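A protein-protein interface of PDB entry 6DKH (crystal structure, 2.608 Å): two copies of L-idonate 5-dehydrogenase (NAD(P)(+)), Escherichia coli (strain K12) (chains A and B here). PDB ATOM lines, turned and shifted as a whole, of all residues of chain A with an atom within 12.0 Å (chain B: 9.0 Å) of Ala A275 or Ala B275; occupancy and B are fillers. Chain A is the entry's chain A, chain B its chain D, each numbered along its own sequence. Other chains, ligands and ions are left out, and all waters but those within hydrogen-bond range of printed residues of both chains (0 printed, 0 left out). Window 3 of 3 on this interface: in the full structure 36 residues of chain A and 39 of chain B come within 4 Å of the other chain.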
ATOM      1  N   GLU A 244      -9.487  -0.827   3.713  1.00  0.00           N
ATOM      2  CA  GLU A 244     -10.591   0.041   3.318  1.00  0.00           C
ATOM      3  C   GLU A 244     -10.658   0.069   1.795  1.00  0.00           C
ATOM      4  O   GLU A 244      -9.742   0.574   1.136  1.00  0.00           O
ATOM      5  CB  GLU A 244     -10.406   1.442   3.894  1.00  0.00           C
ATOM      6  CG  GLU A 244     -11.255   2.509   3.224  1.00  0.00           C
ATOM      7  CD  GLU A 244     -12.739   2.246   3.349  1.00  0.00           C
ATOM      8  OE1 GLU A 244     -13.150   1.607   4.339  1.00  0.00           O
ATOM      9  OE2 GLU A 244     -13.495   2.678   2.455  1.00  0.00           O
ATOM     10  N   GLY A 247     -14.459   3.110   0.104  1.00  0.00           N
ATOM     11  CA  GLY A 247     -14.226   4.529  -0.064  1.00  0.00           C
ATOM     12  C   GLY A 247     -15.182   5.424   0.695  1.00  0.00           C
ATOM     13  O   GLY A 247     -14.968   6.642   0.727  1.00  0.00           O
ATOM     14  N   HIS A 248     -16.223   4.861   1.306  1.00  0.00           N
ATOM     15  CA  HIS A 248     -17.184   5.673   2.039  1.00  0.00           C
ATOM     16  C   HIS A 248     -16.600   6.090   3.387  1.00  0.00           C
ATOM     17  O   HIS A 248     -15.899   5.304   4.029  1.00  0.00           O
ATOM     18  CB  HIS A 248     -18.486   4.905   2.249  1.00  0.00           C
ATOM     19  CG  HIS A 248     -19.049   4.320   0.992  1.00  0.00           C
ATOM     20  ND1 HIS A 248     -19.452   5.094  -0.075  1.00  0.00           N
ATOM     21  CD2 HIS A 248     -19.274   3.035   0.629  1.00  0.00           C
ATOM     22  CE1 HIS A 248     -19.900   4.312  -1.040  1.00  0.00           C
ATOM     23  NE2 HIS A 248     -19.804   3.058  -0.638  1.00  0.00           N
ATOM     24  N   PRO A 249     -16.868   7.323   3.830  1.00  0.00           N
ATOM     25  CA  PRO A 249     -16.295   7.781   5.109  1.00  0.00           C
ATOM     26  C   PRO A 249     -16.695   6.925   6.298  1.00  0.00           C
ATOM     27  O   PRO A 249     -15.876   6.712   7.201  1.00  0.00           O
ATOM     28  CB  PRO A 249     -16.833   9.213   5.231  1.00  0.00           C
ATOM     29  CG  PRO A 249     -17.103   9.635   3.825  1.00  0.00           C
ATOM     30  CD  PRO A 249     -17.585   8.399   3.126  1.00  0.00           C
ATOM     31  N   SER A 250     -17.936   6.431   6.330  1.00  0.00           N
ATOM     32  CA  SER A 250     -18.353   5.555   7.419  1.00  0.00           C
ATOM     33  C   SER A 250     -17.527   4.277   7.451  1.00  0.00           C
ATOM     34  O   SER A 250     -17.258   3.737   8.531  1.00  0.00           O
ATOM     35  CB  SER A 250     -19.840   5.224   7.289  1.00  0.00           C
ATOM     36  OG  SER A 250     -20.107   4.562   6.065  1.00  0.00           O
ATOM     37  N   SER A 251     -17.114   3.783   6.283  1.00  0.00           N
ATOM     38  CA  SER A 251     -16.247   2.612   6.240  1.00  0.00           C
ATOM     39  C   SER A 251     -14.836   2.942   6.709  1.00  0.00           C
ATOM     40  O   SER A 251     -14.160   2.085   7.288  1.00  0.00           O
ATOM     41  CB  SER A 251     -16.224   2.038   4.824  1.00  0.00           C
ATOM     42  OG  SER A 251     -15.302   0.968   4.721  1.00  0.00           O
ATOM     43  N   VAL A 252     -14.376   4.172   6.466  1.00  0.00           N
ATOM     44  CA  VAL A 252     -13.080   4.596   6.986  1.00  0.00           C
ATOM     45  C   VAL A 252     -13.119   4.683   8.507  1.00  0.00           C
ATOM     46  O   VAL A 252     -12.157   4.314   9.190  1.00  0.00           O
ATOM     47  CB  VAL A 252     -12.665   5.935   6.347  1.00  0.00           C
ATOM     48  CG1 VAL A 252     -11.456   6.523   7.060  1.00  0.00           C
ATOM     49  CG2 VAL A 252     -12.371   5.746   4.868  1.00  0.00           C
ATOM     50  N   ASN A 253     -14.236   5.162   9.061  1.00  0.00           N
ATOM     51  CA  ASN A 253     -14.353   5.282  10.510  1.00  0.00           C
ATOM     52  C   ASN A 253     -14.382   3.914  11.182  1.00  0.00           C
ATOM     53  O   ASN A 253     -13.770   3.724  12.239  1.00  0.00           O
ATOM     54  CB  ASN A 253     -15.602   6.084  10.871  1.00  0.00           C
ATOM     55  CG  ASN A 253     -15.559   7.503  10.340  1.00  0.00           C
ATOM     56  OD1 ASN A 253     -14.508   8.144  10.337  1.00  0.00           O
ATOM     57  ND2 ASN A 253     -16.702   8.000   9.884  1.00  0.00           N
ATOM     58  N   THR A 254     -15.086   2.949  10.586  1.00  0.00           N
ATOM     59  CA  THR A 254     -15.153   1.616  11.178  1.00  0.00           C
ATOM     60  C   THR A 254     -13.787   0.942  11.178  1.00  0.00           C
ATOM     61  O   THR A 254     -13.436   0.242  12.135  1.00  0.00           O
ATOM     62  CB  THR A 254     -16.178   0.756  10.434  1.00  0.00           C
ATOM     63  OG1 THR A 254     -15.897   0.775   9.030  1.00  0.00           O
ATOM     64  CG2 THR A 254     -17.591   1.271  10.677  1.00  0.00           C
ATOM     65  N   LEU A 256     -10.911   2.411  11.455  1.00  0.00           N
ATOM     66  CA  LEU A 256     -10.055   3.024  12.466  1.00  0.00           C
ATOM     67  C   LEU A 256     -10.419   2.544  13.866  1.00  0.00           C
ATOM     68  O   LEU A 256      -9.539   2.370  14.716  1.00  0.00           O
ATOM     69  CB  LEU A 256     -10.145   4.548  12.374  1.00  0.00           C
ATOM     70  CG  LEU A 256      -9.403   5.207  11.216  1.00  0.00           C
ATOM     71  CD1 LEU A 256      -9.742   6.688  11.126  1.00  0.00           C
ATOM     72  CD2 LEU A 256      -7.900   5.013  11.368  1.00  0.00           C
ATOM     73  N   MET A 265      -3.628   0.129   8.486  1.00  0.00           N
ATOM     74  CA  MET A 265      -4.842   0.366   7.711  1.00  0.00           C
ATOM     75  C   MET A 265      -4.434   0.681   6.280  1.00  0.00           C
ATOM     76  O   MET A 265      -3.846   1.735   6.016  1.00  0.00           O
ATOM     77  CB  MET A 265      -5.672   1.504   8.308  1.00  0.00           C
ATOM     78  CG  MET A 265      -6.912   1.853   7.502  1.00  0.00           C
ATOM     79  SD  MET A 265      -7.935   3.114   8.286  1.00  0.00           S
ATOM     80  CE  MET A 265      -9.172   3.391   7.019  1.00  0.00           C
ATOM     81  N   GLN A 267      -5.389   1.767   2.686  1.00  0.00           N
ATOM     82  CA  GLN A 267      -6.438   2.528   2.017  1.00  0.00           C
ATOM     83  C   GLN A 267      -6.373   2.243   0.521  1.00  0.00           C
ATOM     84  O   GLN A 267      -5.393   2.595  -0.142  1.00  0.00           O
ATOM     85  CB  GLN A 267      -6.284   4.020   2.300  1.00  0.00           C
ATOM     86  CG  GLN A 267      -7.335   4.881   1.630  1.00  0.00           C
ATOM     87  CD  GLN A 267      -8.703   4.729   2.257  1.00  0.00           C
ATOM     88  OE1 GLN A 267      -8.827   4.554   3.469  1.00  0.00           O
ATOM     89  NE2 GLN A 267      -9.743   4.794   1.432  1.00  0.00           N
ATOM     90  N   GLY A 269      -9.736   2.169  -1.592  1.00  0.00           N
ATOM     91  CA  GLY A 269     -10.824   2.821  -2.298  1.00  0.00           C
ATOM     92  C   GLY A 269     -10.663   4.331  -2.332  1.00  0.00           C
ATOM     93  O   GLY A 269     -10.320   4.968  -1.335  1.00  0.00           O
ATOM     94  N   MET A 270     -10.921   4.906  -3.503  1.00  0.00           N
ATOM     95  CA  MET A 270     -10.893   6.346  -3.706  1.00  0.00           C
ATOM     96  C   MET A 270     -12.321   6.876  -3.694  1.00  0.00           C
ATOM     97  O   MET A 270     -13.195   6.327  -4.372  1.00  0.00           O
ATOM     98  CB  MET A 270     -10.210   6.696  -5.029  1.00  0.00           C
ATOM     99  CG  MET A 270      -8.913   5.940  -5.279  1.00  0.00           C
ATOM    100  SD  MET A 270      -8.325   6.117  -6.975  1.00  0.00           S
ATOM    101  CE  MET A 270      -6.889   5.046  -6.958  1.00  0.00           C
ATOM    102  N   GLY A 271     -12.553   7.936  -2.926  1.00  0.00           N
ATOM    103  CA  GLY A 271     -13.886   8.491  -2.804  1.00  0.00           C
ATOM    104  C   GLY A 271     -13.916   9.980  -2.529  1.00  0.00           C
ATOM    105  O   GLY A 271     -14.754  10.453  -1.757  1.00  0.00           O
ATOM    106  N   GLY A 272     -13.014  10.728  -3.154  1.00  0.00           N
ATOM    107  CA  GLY A 272     -12.968  12.166  -3.007  1.00  0.00           C
ATOM    108  C   GLY A 272     -12.127  12.608  -1.821  1.00  0.00           C
ATOM    109  O   GLY A 272     -11.654  11.808  -1.008  1.00  0.00           O
ATOM    110  N   ALA A 273     -11.932  13.922  -1.736  1.00  0.00           N
ATOM    111  CA  ALA A 273     -11.220  14.530  -0.613  1.00  0.00           C
ATOM    112  C   ALA A 273     -12.038  14.301   0.652  1.00  0.00           C
ATOM    113  O   ALA A 273     -12.974  15.047   0.945  1.00  0.00           O
ATOM    114  CB  ALA A 273     -10.986  16.014  -0.866  1.00  0.00           C
ATOM    115  N   MET A 274     -11.677  13.262   1.401  1.00  0.00           N
ATOM    116  CA  MET A 274     -12.485  12.814   2.529  1.00  0.00           C
ATOM    117  C   MET A 274     -12.599  13.906   3.586  1.00  0.00           C
ATOM    118  O   MET A 274     -11.592  14.419   4.081  1.00  0.00           O
ATOM    119  CB  MET A 274     -11.875  11.545   3.129  1.00  0.00           C
ATOM    120  CG  MET A 274     -12.778  10.799   4.102  1.00  0.00           C
ATOM    121  SD  MET A 274     -12.556  11.306   5.818  1.00  0.00           S
ATOM    122  CE  MET A 274     -13.614  10.134   6.667  1.00  0.00           C
ATOM    123  N   ALA A 275     -13.833  14.259   3.927  1.00  0.00           N
ATOM    124  CA  ALA A 275     -14.120  15.307   4.892  1.00  0.00           C
ATOM    125  C   ALA A 275     -14.419  14.710   6.263  1.00  0.00           C
ATOM    126  O   ALA A 275     -14.789  13.540   6.390  1.00  0.00           O
ATOM    127  CB  ALA A 275     -15.300  16.167   4.428  1.00  0.00           C
ATOM    128  N   GLU A 276     -14.251  15.543   7.293  1.00  0.00           N
ATOM    129  CA  GLU A 276     -14.510  15.154   8.681  1.00  0.00           C
ATOM    130  C   GLU A 276     -13.671  13.942   9.081  1.00  0.00           C
ATOM    131  O   GLU A 276     -14.143  13.032   9.766  1.00  0.00           O
ATOM    132  CB  GLU A 276     -16.001  14.890   8.909  1.00  0.00           C
ATOM    133  CG  GLU A 276     -16.573  15.551  10.153  1.00  0.00           C
ATOM    134  CD  GLU A 276     -18.085  15.435  10.231  1.00  0.00           C
ATOM    135  OE1 GLU A 276     -18.684  16.051  11.138  1.00  0.00           O
ATOM    136  OE2 GLU A 276     -18.674  14.731   9.384  1.00  0.00           O
ATOM    137  N   PHE A 277     -12.417  13.932   8.649  1.00  0.00           N
ATOM    138  CA  PHE A 277     -11.520  12.818   8.938  1.00  0.00           C
ATOM    139  C   PHE A 277     -11.137  12.817  10.413  1.00  0.00           C
ATOM    140  O   PHE A 277     -10.576  13.808  10.897  1.00  0.00           O
ATOM    141  CB  PHE A 277     -10.271  12.907   8.064  1.00  0.00           C
ATOM    142  CG  PHE A 277      -9.228  11.875   8.387  1.00  0.00           C
ATOM    143  CD1 PHE A 277      -9.414  10.548   8.034  1.00  0.00           C
ATOM    144  CD2 PHE A 277      -8.058  12.234   9.036  1.00  0.00           C
ATOM    145  CE1 PHE A 277      -8.455   9.597   8.330  1.00  0.00           C
ATOM    146  CE2 PHE A 277      -7.094  11.286   9.332  1.00  0.00           C
ATOM    147  CZ  PHE A 277      -7.294   9.967   8.979  1.00  0.00           C
ATOM    148  N   PRO A 278     -11.413  11.745  11.159  1.00  0.00           N
ATOM    149  CA  PRO A 278     -11.023  11.686  12.584  1.00  0.00           C
ATOM    150  C   PRO A 278      -9.525  11.451  12.763  1.00  0.00           C
ATOM    151  O   PRO A 278      -9.045  10.355  13.050  1.00  0.00           O
ATOM    152  CB  PRO A 278     -11.858  10.517  13.110  1.00  0.00           C
ATOM    153  CG  PRO A 278     -12.014   9.622  11.928  1.00  0.00           C
ATOM    154  CD  PRO A 278     -12.134  10.533  10.733  1.00  0.00           C
ATOM    155  N   MET A 279      -8.753  12.525  12.579  1.00  0.00           N
ATOM    156  CA  MET A 279      -7.305  12.423  12.723  1.00  0.00           C
ATOM    157  C   MET A 279      -6.904  12.175  14.172  1.00  0.00           C
ATOM    158  O   MET A 279      -5.859  11.566  14.428  1.00  0.00           O
ATOM    159  CB  MET A 279      -6.638  13.687  12.177  1.00  0.00           C
ATOM    160  CG  MET A 279      -5.120  13.700  12.274  1.00  0.00           C
ATOM    161  SD  MET A 279      -4.351  14.775  11.047  1.00  0.00           S
ATOM    162  CE  MET A 279      -4.316  13.690   9.622  1.00  0.00           C
ATOM    163  N   MET A 280      -7.726  12.620  15.127  1.00  0.00           N
ATOM    164  CA  MET A 280      -7.427  12.383  16.536  1.00  0.00           C
ATOM    165  C   MET A 280      -7.375  10.891  16.845  1.00  0.00           C
ATOM    166  O   MET A 280      -6.559  10.446  17.662  1.00  0.00           O
ATOM    167  CB  MET A 280      -8.472  13.073  17.412  1.00  0.00           C
ATOM    168  CG  MET A 280      -8.053  13.258  18.859  1.00  0.00           C
ATOM    169  SD  MET A 280      -6.745  14.486  19.020  1.00  0.00           S
ATOM    170  CE  MET A 280      -7.494  15.876  18.174  1.00  0.00           C
ATOM    171  N   THR A 281      -8.238  10.103  16.199  1.00  0.00           N
ATOM    172  CA  THR A 281      -8.227   8.659  16.411  1.00  0.00           C
ATOM    173  C   THR A 281      -6.948   8.033  15.871  1.00  0.00           C
ATOM    174  O   THR A 281      -6.390   7.116  16.487  1.00  0.00           O
ATOM    175  CB  THR A 281      -9.453   8.021  15.755  1.00  0.00           C
ATOM    176  OG1 THR A 281     -10.643   8.655  16.243  1.00  0.00           O
ATOM    177  CG2 THR A 281      -9.516   6.534  16.069  1.00  0.00           C
ATOM    178  N   ILE A 283      -4.061   9.531  15.640  1.00  0.00           N
ATOM    179  CA  ILE A 283      -2.943   9.959  16.477  1.00  0.00           C
ATOM    180  C   ILE A 283      -2.906   9.153  17.769  1.00  0.00           C
ATOM    181  O   ILE A 283      -1.862   8.607  18.147  1.00  0.00           O
ATOM    182  CB  ILE A 283      -3.032  11.468  16.765  1.00  0.00           C
ATOM    183  CG1 ILE A 283      -2.986  12.270  15.463  1.00  0.00           C
ATOM    184  CG2 ILE A 283      -1.909  11.901  17.698  1.00  0.00           C
ATOM    185  CD1 ILE A 283      -3.225  13.751  15.656  1.00  0.00           C
ATOM    186  N   LEU A 289      -1.413   4.344   8.532  1.00  0.00           N
ATOM    187  CA  LEU A 289      -2.332   4.451   7.404  1.00  0.00           C
ATOM    188  C   LEU A 289      -1.517   4.526   6.118  1.00  0.00           C
ATOM    189  O   LEU A 289      -0.869   5.542   5.844  1.00  0.00           O
ATOM    190  CB  LEU A 289      -3.238   5.671   7.559  1.00  0.00           C
ATOM    191  CG  LEU A 289      -4.229   5.964   6.431  1.00  0.00           C
ATOM    192  CD1 LEU A 289      -5.065   4.738   6.110  1.00  0.00           C
ATOM    193  CD2 LEU A 289      -5.127   7.135   6.804  1.00  0.00           C
ATOM    194  N   GLY B 247      -0.583  20.843  13.709  1.00  0.00           N
ATOM    195  CA  GLY B 247      -1.966  20.433  13.824  1.00  0.00           C
ATOM    196  C   GLY B 247      -2.942  21.223  12.982  1.00  0.00           C
ATOM    197  O   GLY B 247      -4.155  21.029  13.124  1.00  0.00           O
ATOM    198  N   HIS B 248      -2.456  22.107  12.114  1.00  0.00           N
ATOM    199  CA  HIS B 248      -3.278  22.926  11.233  1.00  0.00           C
ATOM    200  C   HIS B 248      -3.548  22.191   9.922  1.00  0.00           C
ATOM    201  O   HIS B 248      -2.639  21.570   9.363  1.00  0.00           O
ATOM    202  CB  HIS B 248      -2.593  24.256  10.937  1.00  0.00           C
ATOM    203  CG  HIS B 248      -2.353  25.095  12.153  1.00  0.00           C
ATOM    204  ND1 HIS B 248      -3.225  25.125  13.220  1.00  0.00           N
ATOM    205  CD2 HIS B 248      -1.336  25.929  12.474  1.00  0.00           C
ATOM    206  CE1 HIS B 248      -2.758  25.945  14.144  1.00  0.00           C
ATOM    207  NE2 HIS B 248      -1.613  26.446  13.718  1.00  0.00           N
ATOM    208  N   PRO B 249      -4.786  22.247   9.425  1.00  0.00           N
ATOM    209  CA  PRO B 249      -5.095  21.565   8.156  1.00  0.00           C
ATOM    210  C   PRO B 249      -4.276  22.074   6.983  1.00  0.00           C
ATOM    211  O   PRO B 249      -3.968  21.295   6.070  1.00  0.00           O
ATOM    212  CB  PRO B 249      -6.592  21.847   7.964  1.00  0.00           C
ATOM    213  CG  PRO B 249      -7.105  22.143   9.338  1.00  0.00           C
ATOM    214  CD  PRO B 249      -5.983  22.845  10.040  1.00  0.00           C
ATOM    215  N   SER B 250      -3.915  23.359   6.976  1.00  0.00           N
ATOM    216  CA  SER B 250      -3.068  23.883   5.909  1.00  0.00           C
ATOM    217  C   SER B 250      -1.695  23.224   5.922  1.00  0.00           C
ATOM    218  O   SER B 250      -1.140  22.905   4.865  1.00  0.00           O
ATOM    219  CB  SER B 250      -2.939  25.399   6.044  1.00  0.00           C
ATOM    220  OG  SER B 250      -1.870  25.896   5.257  1.00  0.00           O
ATOM    221  N   VAL B 252      -1.011  20.252   6.990  1.00  0.00           N
ATOM    222  CA  VAL B 252      -1.102  18.832   6.670  1.00  0.00           C
ATOM    223  C   VAL B 252      -1.037  18.617   5.163  1.00  0.00           C
ATOM    224  O   VAL B 252      -0.414  17.661   4.685  1.00  0.00           O
ATOM    225  CB  VAL B 252      -2.384  18.230   7.276  1.00  0.00           C
ATOM    226  CG1 VAL B 252      -2.494  16.759   6.930  1.00  0.00           C
ATOM    227  CG2 VAL B 252      -2.395  18.416   8.781  1.00  0.00           C
ATOM    228  N   ASN B 253      -1.679  19.497   4.392  1.00  0.00           N
ATOM    229  CA  ASN B 253      -1.613  19.396   2.937  1.00  0.00           C
ATOM    230  C   ASN B 253      -0.184  19.577   2.441  1.00  0.00           C
ATOM    231  O   ASN B 253       0.293  18.811   1.595  1.00  0.00           O
ATOM    232  CB  ASN B 253      -2.541  20.428   2.295  1.00  0.00           C
ATOM    233  CG  ASN B 253      -4.000  20.022   2.361  1.00  0.00           C
ATOM    234  OD1 ASN B 253      -4.591  19.625   1.357  1.00  0.00           O
ATOM    235  ND2 ASN B 253      -4.588  20.118   3.548  1.00  0.00           N
ATOM    236  N   GLY B 271      -5.269  18.764  16.275  1.00  0.00           N
ATOM    237  CA  GLY B 271      -6.101  19.944  16.140  1.00  0.00           C
ATOM    238  C   GLY B 271      -7.531  19.607  15.775  1.00  0.00           C
ATOM    239  O   GLY B 271      -8.042  20.067  14.751  1.00  0.00           O
ATOM    240  N   GLY B 272      -8.188  18.806  16.610  1.00  0.00           N
ATOM    241  CA  GLY B 272      -9.525  18.363  16.282  1.00  0.00           C
ATOM    242  C   GLY B 272      -9.520  17.398  15.103  1.00  0.00           C
ATOM    243  O   GLY B 272      -8.498  16.819  14.728  1.00  0.00           O
ATOM    244  N   ALA B 273     -10.698  17.235  14.514  1.00  0.00           N
ATOM    245  CA  ALA B 273     -10.862  16.406  13.327  1.00  0.00           C
ATOM    246  C   ALA B 273     -10.636  17.257  12.079  1.00  0.00           C
ATOM    247  O   ALA B 273     -11.386  18.207  11.834  1.00  0.00           O
ATOM    248  CB  ALA B 273     -12.254  15.775  13.312  1.00  0.00           C
ATOM    249  N   MET B 274      -9.605  16.922  11.297  1.00  0.00           N
ATOM    250  CA  MET B 274      -9.353  17.643  10.052  1.00  0.00           C
ATOM    251  C   MET B 274     -10.551  17.504   9.120  1.00  0.00           C
ATOM    252  O   MET B 274     -11.052  16.399   8.886  1.00  0.00           O
ATOM    253  CB  MET B 274      -8.081  17.128   9.378  1.00  0.00           C
ATOM    254  CG  MET B 274      -6.984  18.166   9.193  1.00  0.00           C
ATOM    255  SD  MET B 274      -6.401  18.061   7.480  1.00  0.00           S
ATOM    256  CE  MET B 274      -7.918  18.243   6.519  1.00  0.00           C
ATOM    257  N   ALA B 275     -10.999  18.632   8.577  1.00  0.00           N
ATOM    258  CA  ALA B 275     -12.334  18.753   8.013  1.00  0.00           C
ATOM    259  C   ALA B 275     -12.398  18.552   6.502  1.00  0.00           C
ATOM    260  O   ALA B 275     -13.491  18.635   5.937  1.00  0.00           O
ATOM    261  CB  ALA B 275     -12.918  20.120   8.377  1.00  0.00           C
ATOM    262  N   GLU B 276     -11.272  18.293   5.836  1.00  0.00           N
ATOM    263  CA  GLU B 276     -11.275  18.082   4.390  1.00  0.00           C
ATOM    264  C   GLU B 276      -9.977  17.433   3.934  1.00  0.00           C
ATOM    265  O   GLU B 276      -9.162  18.073   3.260  1.00  0.00           O
ATOM    266  CB  GLU B 276     -11.475  19.406   3.648  1.00  0.00           C
ATOM    267  N   PHE B 277      -9.776  16.174   4.286  1.00  0.00           N
ATOM    268  CA  PHE B 277      -8.464  15.575   4.084  1.00  0.00           C
ATOM    269  C   PHE B 277      -8.304  15.118   2.638  1.00  0.00           C
ATOM    270  O   PHE B 277      -9.157  14.382   2.125  1.00  0.00           O
ATOM    271  CB  PHE B 277      -8.259  14.390   5.028  1.00  0.00           C
ATOM    272  CG  PHE B 277      -6.823  13.912   5.114  1.00  0.00           C
ATOM    273  CD1 PHE B 277      -5.801  14.788   5.468  1.00  0.00           C
ATOM    274  CD2 PHE B 277      -6.499  12.588   4.874  1.00  0.00           C
ATOM    275  CE1 PHE B 277      -4.481  14.343   5.561  1.00  0.00           C
ATOM    276  CE2 PHE B 277      -5.180  12.139   4.967  1.00  0.00           C
ATOM    277  CZ  PHE B 277      -4.173  13.020   5.311  1.00  0.00           C
ATOM    278  N   PRO B 278      -7.230  15.527   1.958  1.00  0.00           N
ATOM    279  CA  PRO B 278      -6.959  15.014   0.610  1.00  0.00           C
ATOM    280  C   PRO B 278      -6.567  13.546   0.644  1.00  0.00           C
ATOM    281  O   PRO B 278      -5.388  13.199   0.514  1.00  0.00           O
ATOM    282  CB  PRO B 278      -5.810  15.907   0.118  1.00  0.00           C
ATOM    283  CG  PRO B 278      -5.147  16.398   1.371  1.00  0.00           C
ATOM    284  CD  PRO B 278      -6.247  16.538   2.385  1.00  0.00           C
ATOM    285  N   MET B 279      -7.563  12.675   0.838  1.00  0.00           N
ATOM    286  CA  MET B 279      -7.300  11.241   0.879  1.00  0.00           C
ATOM    287  C   MET B 279      -6.751  10.745  -0.451  1.00  0.00           C
ATOM    288  O   MET B 279      -5.949   9.807  -0.482  1.00  0.00           O
ATOM    289  CB  MET B 279      -8.577  10.485   1.255  1.00  0.00           C
ATOM    290  CG  MET B 279      -8.449   8.967   1.233  1.00  0.00           C
ATOM    291  SD  MET B 279      -7.142   8.353   2.313  1.00  0.00           S
ATOM    292  CE  MET B 279      -7.845   8.671   3.929  1.00  0.00           C
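NE2 of Gln A267 sits at hydrogen-bond distance from O of Gly A269 (2.8 Å).
Of the 27 printed residues of chain A, 7 touch a printed residue of chain B. Printed residues of chain A that touch a printed residue of chain B: Gln A267, Ala A273, Met A274, Ala A275, Glu A276, Phe A277 and Met A280. Of the 15 printed residues of chain B, 7 touch a printed residue of chain A. Printed residues of chain B that touch a printed residue of chain A: Gly B272, Ala B273, Met B274, Ala B275, Glu B276, Phe B277 and Met B279. Hydrophobic or aromatic side chains of chain B that line the printed part of chain A: Ala B273, Phe B277 and Met B279.
Of the printed residues of chain B, Ala A275 touches Ala B275 (3.4 Å). Pro B249 touches none of the printed residues of chain A. Met B274 touches just these residues of chain A: Glu A276 and Phe A277. Of the printed residues of chain A, Glu B276 touches Met A274 (3.4 Å). Of the printed residues of chain A, Gly B272 touches Met A280. Printed residues of chain B within 4 Å of Gln A267: Met B279. Gly A271 touches none of the printed residues of chain B. Val A252 touches none of the printed residues of chain B. The nearest printed residue of chain B that does not touch Ala A275 is Glu B276 (4.01 Å). The nearest printed residue of chain A that does not touch Phe B277 is Met A279 (4.1 Å).
Ala A273 touches Phe B277, and with the chains exchanged Phe A277 touches Ala B273. Met A274 touches Glu B276, and with the chains exchanged Glu A276 touches Met B274. Met A274 touches Met B279, but with the chains exchanged Met A279 does not touch Met B274 (4.5 Å). Ala A275 touches its own counterpart, Ala B275.
The backbone carbonyl oxygen of Met B274 lies within hydrogen-bond range of the backbone NH of Phe A277 (2.8 Å). The backbone carbonyl oxygen (O) of Ala B275 is in hydrogen-bond range of the backbone NH (N) of Glu A276 (3.5 Å). The backbone carbonyl oxygen (O) of Met A274 is in hydrogen-bond range of the backbone NH (N) of Phe B277 (2.5 Å).
Among the printed residues, merely in contact across the chains: Gln A267 with Met B279 (3.5 Å), Ala A273 with Phe B277 (3.2 Å), Met A274 with Glu B276 (3.4 Å), Met A274 with Met B279 (3.9 Å), Ala A275 with Ala B275 (3.4 Å), Glu A276 with Met B274 (3.6 Å), Phe A277 with Ala B273 (3.5 Å), Phe A277 with Phe B277 (3.9 Å) and Met A280 with Gly B272 (3.4 Å).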
